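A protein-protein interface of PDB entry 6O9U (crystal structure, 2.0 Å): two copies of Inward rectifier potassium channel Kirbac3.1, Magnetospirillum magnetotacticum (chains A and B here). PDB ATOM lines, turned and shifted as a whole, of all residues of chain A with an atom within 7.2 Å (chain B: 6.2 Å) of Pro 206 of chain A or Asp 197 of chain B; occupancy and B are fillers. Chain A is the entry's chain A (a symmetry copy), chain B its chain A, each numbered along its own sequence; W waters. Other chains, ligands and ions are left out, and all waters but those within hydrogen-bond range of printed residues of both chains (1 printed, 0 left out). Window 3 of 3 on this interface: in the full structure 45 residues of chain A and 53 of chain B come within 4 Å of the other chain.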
ATOM      1  N   ILE A 171     -10.256 -15.616 -13.392  1.00  0.00           N
ATOM      2  CA  ILE A 171     -10.952 -14.410 -13.824  1.00  0.00           C
ATOM      3  C   ILE A 171     -10.676 -14.205 -15.307  1.00  0.00           C
ATOM      4  O   ILE A 171      -9.514 -14.164 -15.732  1.00  0.00           O
ATOM      5  CB  ILE A 171     -10.530 -13.187 -12.992  1.00  0.00           C
ATOM      6  CG1 ILE A 171     -10.718 -13.497 -11.500  1.00  0.00           C
ATOM      7  CG2 ILE A 171     -11.360 -11.976 -13.389  1.00  0.00           C
ATOM      8  CD1 ILE A 171     -10.363 -12.366 -10.549  1.00  0.00           C
ATOM      9  N   ILE A 172     -11.751 -14.059 -16.087  1.00  0.00           N
ATOM     10  CA  ILE A 172     -11.711 -14.119 -17.545  1.00  0.00           C
ATOM     11  C   ILE A 172     -11.688 -12.711 -18.119  1.00  0.00           C
ATOM     12  O   ILE A 172     -12.376 -11.810 -17.619  1.00  0.00           O
ATOM     13  CB  ILE A 172     -12.919 -14.914 -18.080  1.00  0.00           C
ATOM     14  CG1 ILE A 172     -13.042 -16.258 -17.353  1.00  0.00           C
ATOM     15  CG2 ILE A 172     -12.811 -15.128 -19.578  1.00  0.00           C
ATOM     16  CD1 ILE A 172     -11.799 -17.125 -17.422  1.00  0.00           C
ATOM     17  N   GLU A 173     -10.906 -12.525 -19.184  1.00  0.00           N
ATOM     18  CA  GLU A 173     -10.750 -11.235 -19.856  1.00  0.00           C
ATOM     19  C   GLU A 173     -10.477 -10.131 -18.837  1.00  0.00           C
ATOM     20  O   GLU A 173     -11.182  -9.124 -18.753  1.00  0.00           O
ATOM     21  CB  GLU A 173     -11.978 -10.910 -20.711  1.00  0.00           C
ATOM     22  CG  GLU A 173     -12.253 -11.907 -21.832  1.00  0.00           C
ATOM     23  CD  GLU A 173     -11.355 -11.710 -23.037  1.00  0.00           C
ATOM     24  OE1 GLU A 173     -11.861 -11.804 -24.177  1.00  0.00           O
ATOM     25  OE2 GLU A 173     -10.148 -11.455 -22.849  1.00  0.00           O
ATOM     26  N   ALA A 174      -9.420 -10.344 -18.058  1.00  0.00           N
ATOM     27  CA  ALA A 174      -9.059  -9.418 -16.996  1.00  0.00           C
ATOM     28  C   ALA A 174      -8.326  -8.212 -17.568  1.00  0.00           C
ATOM     29  O   ALA A 174      -7.399  -8.357 -18.369  1.00  0.00           O
ATOM     30  CB  ALA A 174      -8.190 -10.124 -15.956  1.00  0.00           C
ATOM     31  N   ARG A 202       1.328  -5.409 -20.677  1.00  0.00           N
ATOM     32  CA  ARG A 202       0.106  -6.196 -20.782  1.00  0.00           C
ATOM     33  C   ARG A 202      -0.992  -5.469 -20.023  1.00  0.00           C
ATOM     34  O   ARG A 202      -0.896  -5.298 -18.803  1.00  0.00           O
ATOM     35  CB  ARG A 202       0.290  -7.610 -20.216  1.00  0.00           C
ATOM     36  CG  ARG A 202       1.394  -8.426 -20.873  1.00  0.00           C
ATOM     37  CD  ARG A 202       1.059  -8.798 -22.310  1.00  0.00           C
ATOM     38  NE  ARG A 202       2.049  -9.716 -22.871  1.00  0.00           N
ATOM     39  CZ  ARG A 202       3.189  -9.345 -23.451  1.00  0.00           C
ATOM     40  NH1 ARG A 202       3.507  -8.063 -23.561  1.00  0.00           N
ATOM     41  NH2 ARG A 202       4.018 -10.264 -23.925  1.00  0.00           N
ATOM     42  N   ARG A 204      -4.290  -6.565 -20.768  1.00  0.00           N
ATOM     43  CA  ARG A 204      -5.340  -7.573 -20.806  1.00  0.00           C
ATOM     44  C   ARG A 204      -4.719  -8.936 -20.558  1.00  0.00           C
ATOM     45  O   ARG A 204      -3.739  -9.304 -21.212  1.00  0.00           O
ATOM     46  CB  ARG A 204      -6.071  -7.542 -22.159  1.00  0.00           C
ATOM     47  CG  ARG A 204      -6.885  -8.790 -22.518  1.00  0.00           C
ATOM     48  CD  ARG A 204      -8.077  -8.992 -21.598  1.00  0.00           C
ATOM     49  NE  ARG A 204      -9.004  -7.861 -21.644  1.00  0.00           N
ATOM     50  CZ  ARG A 204      -9.997  -7.725 -22.518  1.00  0.00           C
ATOM     51  NH1 ARG A 204     -10.220  -8.648 -23.444  1.00  0.00           N
ATOM     52  NH2 ARG A 204     -10.777  -6.654 -22.466  1.00  0.00           N
ATOM     53  N   SER A 205      -5.279  -9.669 -19.603  1.00  0.00           N
ATOM     54  CA  SER A 205      -4.937 -11.069 -19.400  1.00  0.00           C
ATOM     55  C   SER A 205      -6.165 -11.907 -19.724  1.00  0.00           C
ATOM     56  O   SER A 205      -7.170 -11.821 -18.997  1.00  0.00           O
ATOM     57  CB  SER A 205      -4.481 -11.323 -17.962  1.00  0.00           C
ATOM     58  OG  SER A 205      -4.106 -12.676 -17.786  1.00  0.00           O
ATOM     59  N   PRO A 206      -6.159 -12.700 -20.800  1.00  0.00           N
ATOM     60  CA  PRO A 206      -7.355 -13.500 -21.117  1.00  0.00           C
ATOM     61  C   PRO A 206      -7.827 -14.371 -19.967  1.00  0.00           C
ATOM     62  O   PRO A 206      -9.040 -14.528 -19.775  1.00  0.00           O
ATOM     63  CB  PRO A 206      -6.898 -14.334 -22.321  1.00  0.00           C
ATOM     64  CG  PRO A 206      -5.863 -13.495 -22.978  1.00  0.00           C
ATOM     65  CD  PRO A 206      -5.141 -12.786 -21.863  1.00  0.00           C
ATOM     66  N   ILE A 207      -6.907 -14.941 -19.191  1.00  0.00           N
ATOM     67  CA  ILE A 207      -7.259 -15.706 -18.001  1.00  0.00           C
ATOM     68  C   ILE A 207      -6.276 -15.324 -16.903  1.00  0.00           C
ATOM     69  O   ILE A 207      -5.112 -15.742 -16.936  1.00  0.00           O
ATOM     70  CB  ILE A 207      -7.243 -17.225 -18.236  1.00  0.00           C
ATOM     71  CG1 ILE A 207      -8.205 -17.595 -19.369  1.00  0.00           C
ATOM     72  CG2 ILE A 207      -7.615 -17.955 -16.942  1.00  0.00           C
ATOM     73  CD1 ILE A 207      -8.362 -19.090 -19.615  1.00  0.00           C
ATOM     74  N   PHE A 208      -6.735 -14.531 -15.939  1.00  0.00           N
ATOM     75  CA  PHE A 208      -5.969 -14.262 -14.730  1.00  0.00           C
ATOM     76  C   PHE A 208      -6.181 -15.420 -13.762  1.00  0.00           C
ATOM     77  O   PHE A 208      -7.319 -15.714 -13.378  1.00  0.00           O
ATOM     78  CB  PHE A 208      -6.406 -12.933 -14.120  1.00  0.00           C
ATOM     79  CG  PHE A 208      -5.800 -12.645 -12.779  1.00  0.00           C
ATOM     80  CD1 PHE A 208      -4.449 -12.366 -12.656  1.00  0.00           C
ATOM     81  CD2 PHE A 208      -6.586 -12.636 -11.639  1.00  0.00           C
ATOM     82  CE1 PHE A 208      -3.895 -12.095 -11.420  1.00  0.00           C
ATOM     83  CE2 PHE A 208      -6.035 -12.364 -10.402  1.00  0.00           C
ATOM     84  CZ  PHE A 208      -4.689 -12.093 -10.294  1.00  0.00           C
ATOM     85  N   TRP A 212      -0.030 -11.669 -11.264  1.00  0.00           N
ATOM     86  CA  TRP A 212       0.163 -10.862 -12.463  1.00  0.00           C
ATOM     87  C   TRP A 212       0.952  -9.617 -12.085  1.00  0.00           C
ATOM     88  O   TRP A 212       0.510  -8.833 -11.240  1.00  0.00           O
ATOM     89  CB  TRP A 212      -1.193 -10.493 -13.075  1.00  0.00           C
ATOM     90  CG  TRP A 212      -1.144  -9.747 -14.376  1.00  0.00           C
ATOM     91  CD1 TRP A 212      -0.045  -9.479 -15.143  1.00  0.00           C
ATOM     92  CD2 TRP A 212      -2.262  -9.172 -15.066  1.00  0.00           C
ATOM     93  NE1 TRP A 212      -0.411  -8.769 -16.264  1.00  0.00           N
ATOM     94  CE2 TRP A 212      -1.768  -8.568 -16.239  1.00  0.00           C
ATOM     95  CE3 TRP A 212      -3.633  -9.109 -14.802  1.00  0.00           C
ATOM     96  CZ2 TRP A 212      -2.596  -7.911 -17.145  1.00  0.00           C
ATOM     97  CZ3 TRP A 212      -4.453  -8.455 -15.702  1.00  0.00           C
ATOM     98  CH2 TRP A 212      -3.933  -7.865 -16.859  1.00  0.00           C
ATOM     99  N   HIS A 246     -14.140 -10.951 -15.532  1.00  0.00           N
ATOM    100  CA  HIS A 246     -15.325 -11.796 -15.409  1.00  0.00           C
ATOM    101  C   HIS A 246     -14.970 -12.991 -14.531  1.00  0.00           C
ATOM    102  O   HIS A 246     -14.217 -13.875 -14.952  1.00  0.00           O
ATOM    103  CB  HIS A 246     -15.801 -12.243 -16.790  1.00  0.00           C
ATOM    104  CG  HIS A 246     -17.053 -13.058 -16.765  1.00  0.00           C
ATOM    105  ND1 HIS A 246     -17.049 -14.424 -16.578  1.00  0.00           N
ATOM    106  CD2 HIS A 246     -18.350 -12.703 -16.919  1.00  0.00           C
ATOM    107  CE1 HIS A 246     -18.291 -14.874 -16.611  1.00  0.00           C
ATOM    108  NE2 HIS A 246     -19.099 -13.848 -16.815  1.00  0.00           N
ATOM    109  N   VAL B 176     -11.929 -14.961 -29.388  1.00  0.00           N
ATOM    110  CA  VAL B 176     -11.024 -16.069 -29.117  1.00  0.00           C
ATOM    111  C   VAL B 176      -9.613 -15.529 -28.944  1.00  0.00           C
ATOM    112  O   VAL B 176      -9.223 -14.535 -29.565  1.00  0.00           O
ATOM    113  CB  VAL B 176     -11.069 -17.147 -30.226  1.00  0.00           C
ATOM    114  CG1 VAL B 176     -10.559 -16.598 -31.550  1.00  0.00           C
ATOM    115  CG2 VAL B 176     -10.278 -18.370 -29.796  1.00  0.00           C
ATOM    116  N   HIS B 177      -8.852 -16.198 -28.082  1.00  0.00           N
ATOM    117  CA  HIS B 177      -7.454 -15.877 -27.838  1.00  0.00           C
ATOM    118  C   HIS B 177      -6.635 -17.153 -27.958  1.00  0.00           C
ATOM    119  O   HIS B 177      -7.018 -18.191 -27.408  1.00  0.00           O
ATOM    120  CB  HIS B 177      -7.244 -15.271 -26.444  1.00  0.00           C
ATOM    121  CG  HIS B 177      -8.115 -14.089 -26.153  1.00  0.00           C
ATOM    122  ND1 HIS B 177      -7.656 -12.791 -26.221  1.00  0.00           N
ATOM    123  CD2 HIS B 177      -9.411 -14.009 -25.768  1.00  0.00           C
ATOM    124  CE1 HIS B 177      -8.635 -11.964 -25.900  1.00  0.00           C
ATOM    125  NE2 HIS B 177      -9.709 -12.677 -25.619  1.00  0.00           N
ATOM    126  N   LEU B 178      -5.530 -17.080 -28.693  1.00  0.00           N
ATOM    127  CA  LEU B 178      -4.474 -18.084 -28.641  1.00  0.00           C
ATOM    128  C   LEU B 178      -3.312 -17.477 -27.868  1.00  0.00           C
ATOM    129  O   LEU B 178      -2.713 -16.493 -28.317  1.00  0.00           O
ATOM    130  CB  LEU B 178      -4.027 -18.511 -30.039  1.00  0.00           C
ATOM    131  CG  LEU B 178      -5.074 -19.129 -30.971  1.00  0.00           C
ATOM    132  CD1 LEU B 178      -4.394 -19.664 -32.224  1.00  0.00           C
ATOM    133  CD2 LEU B 178      -5.859 -20.234 -30.279  1.00  0.00           C
ATOM    134  N   VAL B 179      -3.002 -18.054 -26.712  1.00  0.00           N
ATOM    135  CA  VAL B 179      -2.052 -17.476 -25.770  1.00  0.00           C
ATOM    136  C   VAL B 179      -0.854 -18.407 -25.651  1.00  0.00           C
ATOM    137  O   VAL B 179      -0.995 -19.557 -25.215  1.00  0.00           O
ATOM    138  CB  VAL B 179      -2.700 -17.238 -24.397  1.00  0.00           C
ATOM    139  CG1 VAL B 179      -1.718 -16.574 -23.444  1.00  0.00           C
ATOM    140  CG2 VAL B 179      -3.954 -16.386 -24.548  1.00  0.00           C
ATOM    141  N   LEU B 180       0.318 -17.913 -26.041  1.00  0.00           N
ATOM    142  CA  LEU B 180       1.569 -18.613 -25.785  1.00  0.00           C
ATOM    143  C   LEU B 180       2.047 -18.303 -24.376  1.00  0.00           C
ATOM    144  O   LEU B 180       2.093 -17.137 -23.973  1.00  0.00           O
ATOM    145  CB  LEU B 180       2.637 -18.193 -26.797  1.00  0.00           C
ATOM    146  CG  LEU B 180       4.085 -18.603 -26.491  1.00  0.00           C
ATOM    147  CD1 LEU B 180       4.276 -20.108 -26.615  1.00  0.00           C
ATOM    148  CD2 LEU B 180       5.050 -17.861 -27.395  1.00  0.00           C
ATOM    149  N   PHE B 195       3.144 -14.444 -20.900  1.00  0.00           N
ATOM    150  CA  PHE B 195       2.200 -14.868 -21.920  1.00  0.00           C
ATOM    151  C   PHE B 195       2.205 -13.888 -23.086  1.00  0.00           C
ATOM    152  O   PHE B 195       2.489 -12.697 -22.925  1.00  0.00           O
ATOM    153  CB  PHE B 195       0.775 -15.021 -21.349  1.00  0.00           C
ATOM    154  CG  PHE B 195       0.166 -13.742 -20.843  1.00  0.00           C
ATOM    155  CD1 PHE B 195      -0.541 -12.908 -21.698  1.00  0.00           C
ATOM    156  CD2 PHE B 195       0.271 -13.388 -19.507  1.00  0.00           C
ATOM    157  CE1 PHE B 195      -1.113 -11.735 -21.232  1.00  0.00           C
ATOM    158  CE2 PHE B 195      -0.297 -12.216 -19.035  1.00  0.00           C
ATOM    159  CZ  PHE B 195      -0.991 -11.390 -19.898  1.00  0.00           C
ATOM    160  N   HIS B 196       1.918 -14.421 -24.272  1.00  0.00           N
ATOM    161  CA  HIS B 196       1.752 -13.642 -25.492  1.00  0.00           C
ATOM    162  C   HIS B 196       0.378 -13.954 -26.062  1.00  0.00           C
ATOM    163  O   HIS B 196       0.095 -15.109 -26.401  1.00  0.00           O
ATOM    164  CB  HIS B 196       2.829 -13.976 -26.528  1.00  0.00           C
ATOM    165  CG  HIS B 196       4.228 -13.706 -26.073  1.00  0.00           C
ATOM    166  ND1 HIS B 196       4.880 -12.521 -26.339  1.00  0.00           N
ATOM    167  CD2 HIS B 196       5.110 -14.477 -25.394  1.00  0.00           C
ATOM    168  CE1 HIS B 196       6.098 -12.568 -25.828  1.00  0.00           C
ATOM    169  NE2 HIS B 196       6.263 -13.745 -25.251  1.00  0.00           N
ATOM    170  N   ASP B 197      -0.476 -12.939 -26.158  1.00  0.00           N
ATOM    171  CA  ASP B 197      -1.768 -13.091 -26.820  1.00  0.00           C
ATOM    172  C   ASP B 197      -1.534 -12.952 -28.320  1.00  0.00           C
ATOM    173  O   ASP B 197      -1.311 -11.847 -28.819  1.00  0.00           O
ATOM    174  CB  ASP B 197      -2.764 -12.057 -26.302  1.00  0.00           C
ATOM    175  CG  ASP B 197      -4.212 -12.469 -26.538  1.00  0.00           C
ATOM    176  OD1 ASP B 197      -4.444 -13.549 -27.120  1.00  0.00           O
ATOM    177  OD2 ASP B 197      -5.121 -11.715 -26.131  1.00  0.00           O
ATOM    178  N   LEU B 198      -1.576 -14.075 -29.036  1.00  0.00           N
ATOM    179  CA  LEU B 198      -1.078 -14.112 -30.405  1.00  0.00           C
ATOM    180  C   LEU B 198      -2.037 -13.427 -31.373  1.00  0.00           C
ATOM    181  O   LEU B 198      -3.260 -13.504 -31.228  1.00  0.00           O
ATOM    182  CB  LEU B 198      -0.848 -15.560 -30.841  1.00  0.00           C
ATOM    183  CG  LEU B 198       0.124 -16.379 -29.986  1.00  0.00           C
ATOM    184  CD1 LEU B 198       0.131 -17.837 -30.434  1.00  0.00           C
ATOM    185  CD2 LEU B 198       1.527 -15.797 -30.049  1.00  0.00           C
ATOM    186  N   THR B 199      -1.463 -12.763 -32.375  1.00  0.00           N
ATOM    187  CA  THR B 199      -2.253 -12.115 -33.415  1.00  0.00           C
ATOM    188  C   THR B 199      -2.943 -13.166 -34.273  1.00  0.00           C
ATOM    189  O   THR B 199      -2.305 -14.108 -34.752  1.00  0.00           O
ATOM    190  CB  THR B 199      -1.356 -11.230 -34.284  1.00  0.00           C
ATOM    191  OG1 THR B 199      -0.730 -10.238 -33.465  1.00  0.00           O
ATOM    192  CG2 THR B 199      -2.156 -10.538 -35.375  1.00  0.00           C
ATOM    193  N   LEU B 200      -4.246 -12.997 -34.472  1.00  0.00           N
ATOM    194  CA  LEU B 200      -5.061 -13.955 -35.198  1.00  0.00           C
ATOM    195  C   LEU B 200      -5.594 -13.326 -36.477  1.00  0.00           C
ATOM    196  O   LEU B 200      -5.756 -12.107 -36.571  1.00  0.00           O
ATOM    197  CB  LEU B 200      -6.232 -14.440 -34.334  1.00  0.00           C
ATOM    198  CG  LEU B 200      -5.866 -15.052 -32.981  1.00  0.00           C
ATOM    199  CD1 LEU B 200      -7.121 -15.467 -32.222  1.00  0.00           C
ATOM    200  CD2 LEU B 200      -4.928 -16.242 -33.155  1.00  0.00           C
ATOM    201  N   LEU B 240      -2.565 -21.706 -24.503  1.00  0.00           N
ATOM    202  CA  LEU B 240      -3.843 -21.600 -23.821  1.00  0.00           C
ATOM    203  C   LEU B 240      -4.833 -20.922 -24.756  1.00  0.00           C
ATOM    204  O   LEU B 240      -4.506 -19.905 -25.378  1.00  0.00           O
ATOM    205  CB  LEU B 240      -3.687 -20.801 -22.524  1.00  0.00           C
ATOM    206  CG  LEU B 240      -4.936 -20.495 -21.698  1.00  0.00           C
ATOM    207  CD1 LEU B 240      -5.573 -21.770 -21.178  1.00  0.00           C
ATOM    208  CD2 LEU B 240      -4.551 -19.569 -20.554  1.00  0.00           C
ATOM    209  N   LEU B 242      -8.699 -19.288 -25.049  1.00  0.00           N
ATOM    210  CA  LEU B 242      -9.888 -18.777 -24.380  1.00  0.00           C
ATOM    211  C   LEU B 242     -10.924 -18.402 -25.425  1.00  0.00           C
ATOM    212  O   LEU B 242     -10.620 -17.670 -26.372  1.00  0.00           O
ATOM    213  CB  LEU B 242      -9.575 -17.557 -23.512  1.00  0.00           C
ATOM    214  CG  LEU B 242     -10.811 -16.921 -22.852  1.00  0.00           C
ATOM    215  CD1 LEU B 242     -11.359 -17.811 -21.737  1.00  0.00           C
ATOM    216  CD2 LEU B 242     -10.492 -15.534 -22.341  1.00  0.00           C
HETATM  217  O   HOH W   1      -0.342 -10.314 -25.012  1.00  0.00           O
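N of Val 179 of chain B is in hydrogen-bond range of O of Leu 240 of chain B (2.7 Å).
The backbone carbonyl oxygen (O) of Leu 180 of chain B lies within hydrogen-bond range of the backbone NH (N) of His 196 of chain B, 2.7 Å away.
NH1 of Arg 204 of chain A is in salt-bridge range of OE2 of Glu 173 of chain A.
N of Glu 173 of chain A sits at hydrogen-bond distance from O of Pro 206 of chain A (2.8 Å).
N of Ser 205 of chain A sits at hydrogen-bond distance from O of Ala 174 of chain A, 2.8 Å away.
The backbone carbonyl oxygen of Ile 207 of chain A is in hydrogen-bond range of the side-chain hydroxyl of Ser 205 of chain A (3.3 Å).
Pro 206 of chain A touches just these residues of chain B: His 177 (3.8 Å), Val 179 (3.8 Å), Asp 197 (3.7 Å) and Leu 242 (3.1 Å).
Of chain A, only Pro 206 (3.7 Å) comes within 4 Å of Asp 197 of chain B.
Printed residues of chain A within 4 Å of His 196 of chain B: Arg 202.
Printed residues of chain A within 4 Å of Leu 240 of chain B: Ile 207.
Of the printed residues of chain B, Glu 173 of chain A touches His 177 and Leu 242.
Printed residues of chain A within 4 Å of Leu 242 of chain B: Ile 172, Glu 173, Pro 206 and Ile 207.
Leu 198 of chain B touches none of the printed residues of chain A.
The nearest residue of chain B that does not touch Pro 206 of chain A is Phe 195 of chain B (4.2 Å).
Among the printed residues, pairs that only touch across the chains: Pro 206 of chain A with Leu 242 of chain B (3.1 Å), Arg 204 of chain A with Phe 195 of chain B (3.6 Å), Ile 172 of chain A with Leu 242 of chain B (3.6 Å), Pro 206 of chain A with Asp 197 of chain B (3.7 Å), Pro 206 of chain A with His 177 of chain B (3.8 Å), Pro 206 of chain A with Val 179 of chain B (3.8 Å), Ile 207 of chain A with Leu 242 of chain B (3.9 Å), Ile 207 of chain A with Leu 240 of chain B (3.95 Å), Ser 205 of chain A with Phe 195 of chain B (3.98 Å) and Glu 173 of chain A with Leu 242 of chain B (3.98 Å).
Water W1 lies within hydrogen-bond range of the backbone NH of Asp 197 of chain B (2.9 Å) and the guanidinium group of Arg 202 of chain A (3.3 Å).
No position is printed for both chains.
A ring nitrogen (NE2) of His 177 of chain B sits at hydrogen-bond distance from the side-chain carboxylate (OE1) of Glu 173 of chain A, at 2.7 Å.
O of Phe 195 of chain B lies within hydrogen-bond range of NE of Arg 202 of chain A (3.0 Å).
A ring nitrogen (ND1) of His 196 of chain B is in hydrogen-bond range of the guanidinium group (NH2) of Arg 202 of chain A, at 3.4 Å.
Of the 12 printed residues of chain A, 7 touch a printed residue of chain B.
Printed residues of chain B that touch a printed residue of chain A: His 177, Val 179, Phe 195, His 196, Asp 197, Leu 240 and Leu 242.
Among the printed residues, 13 pairs touch across the chains.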
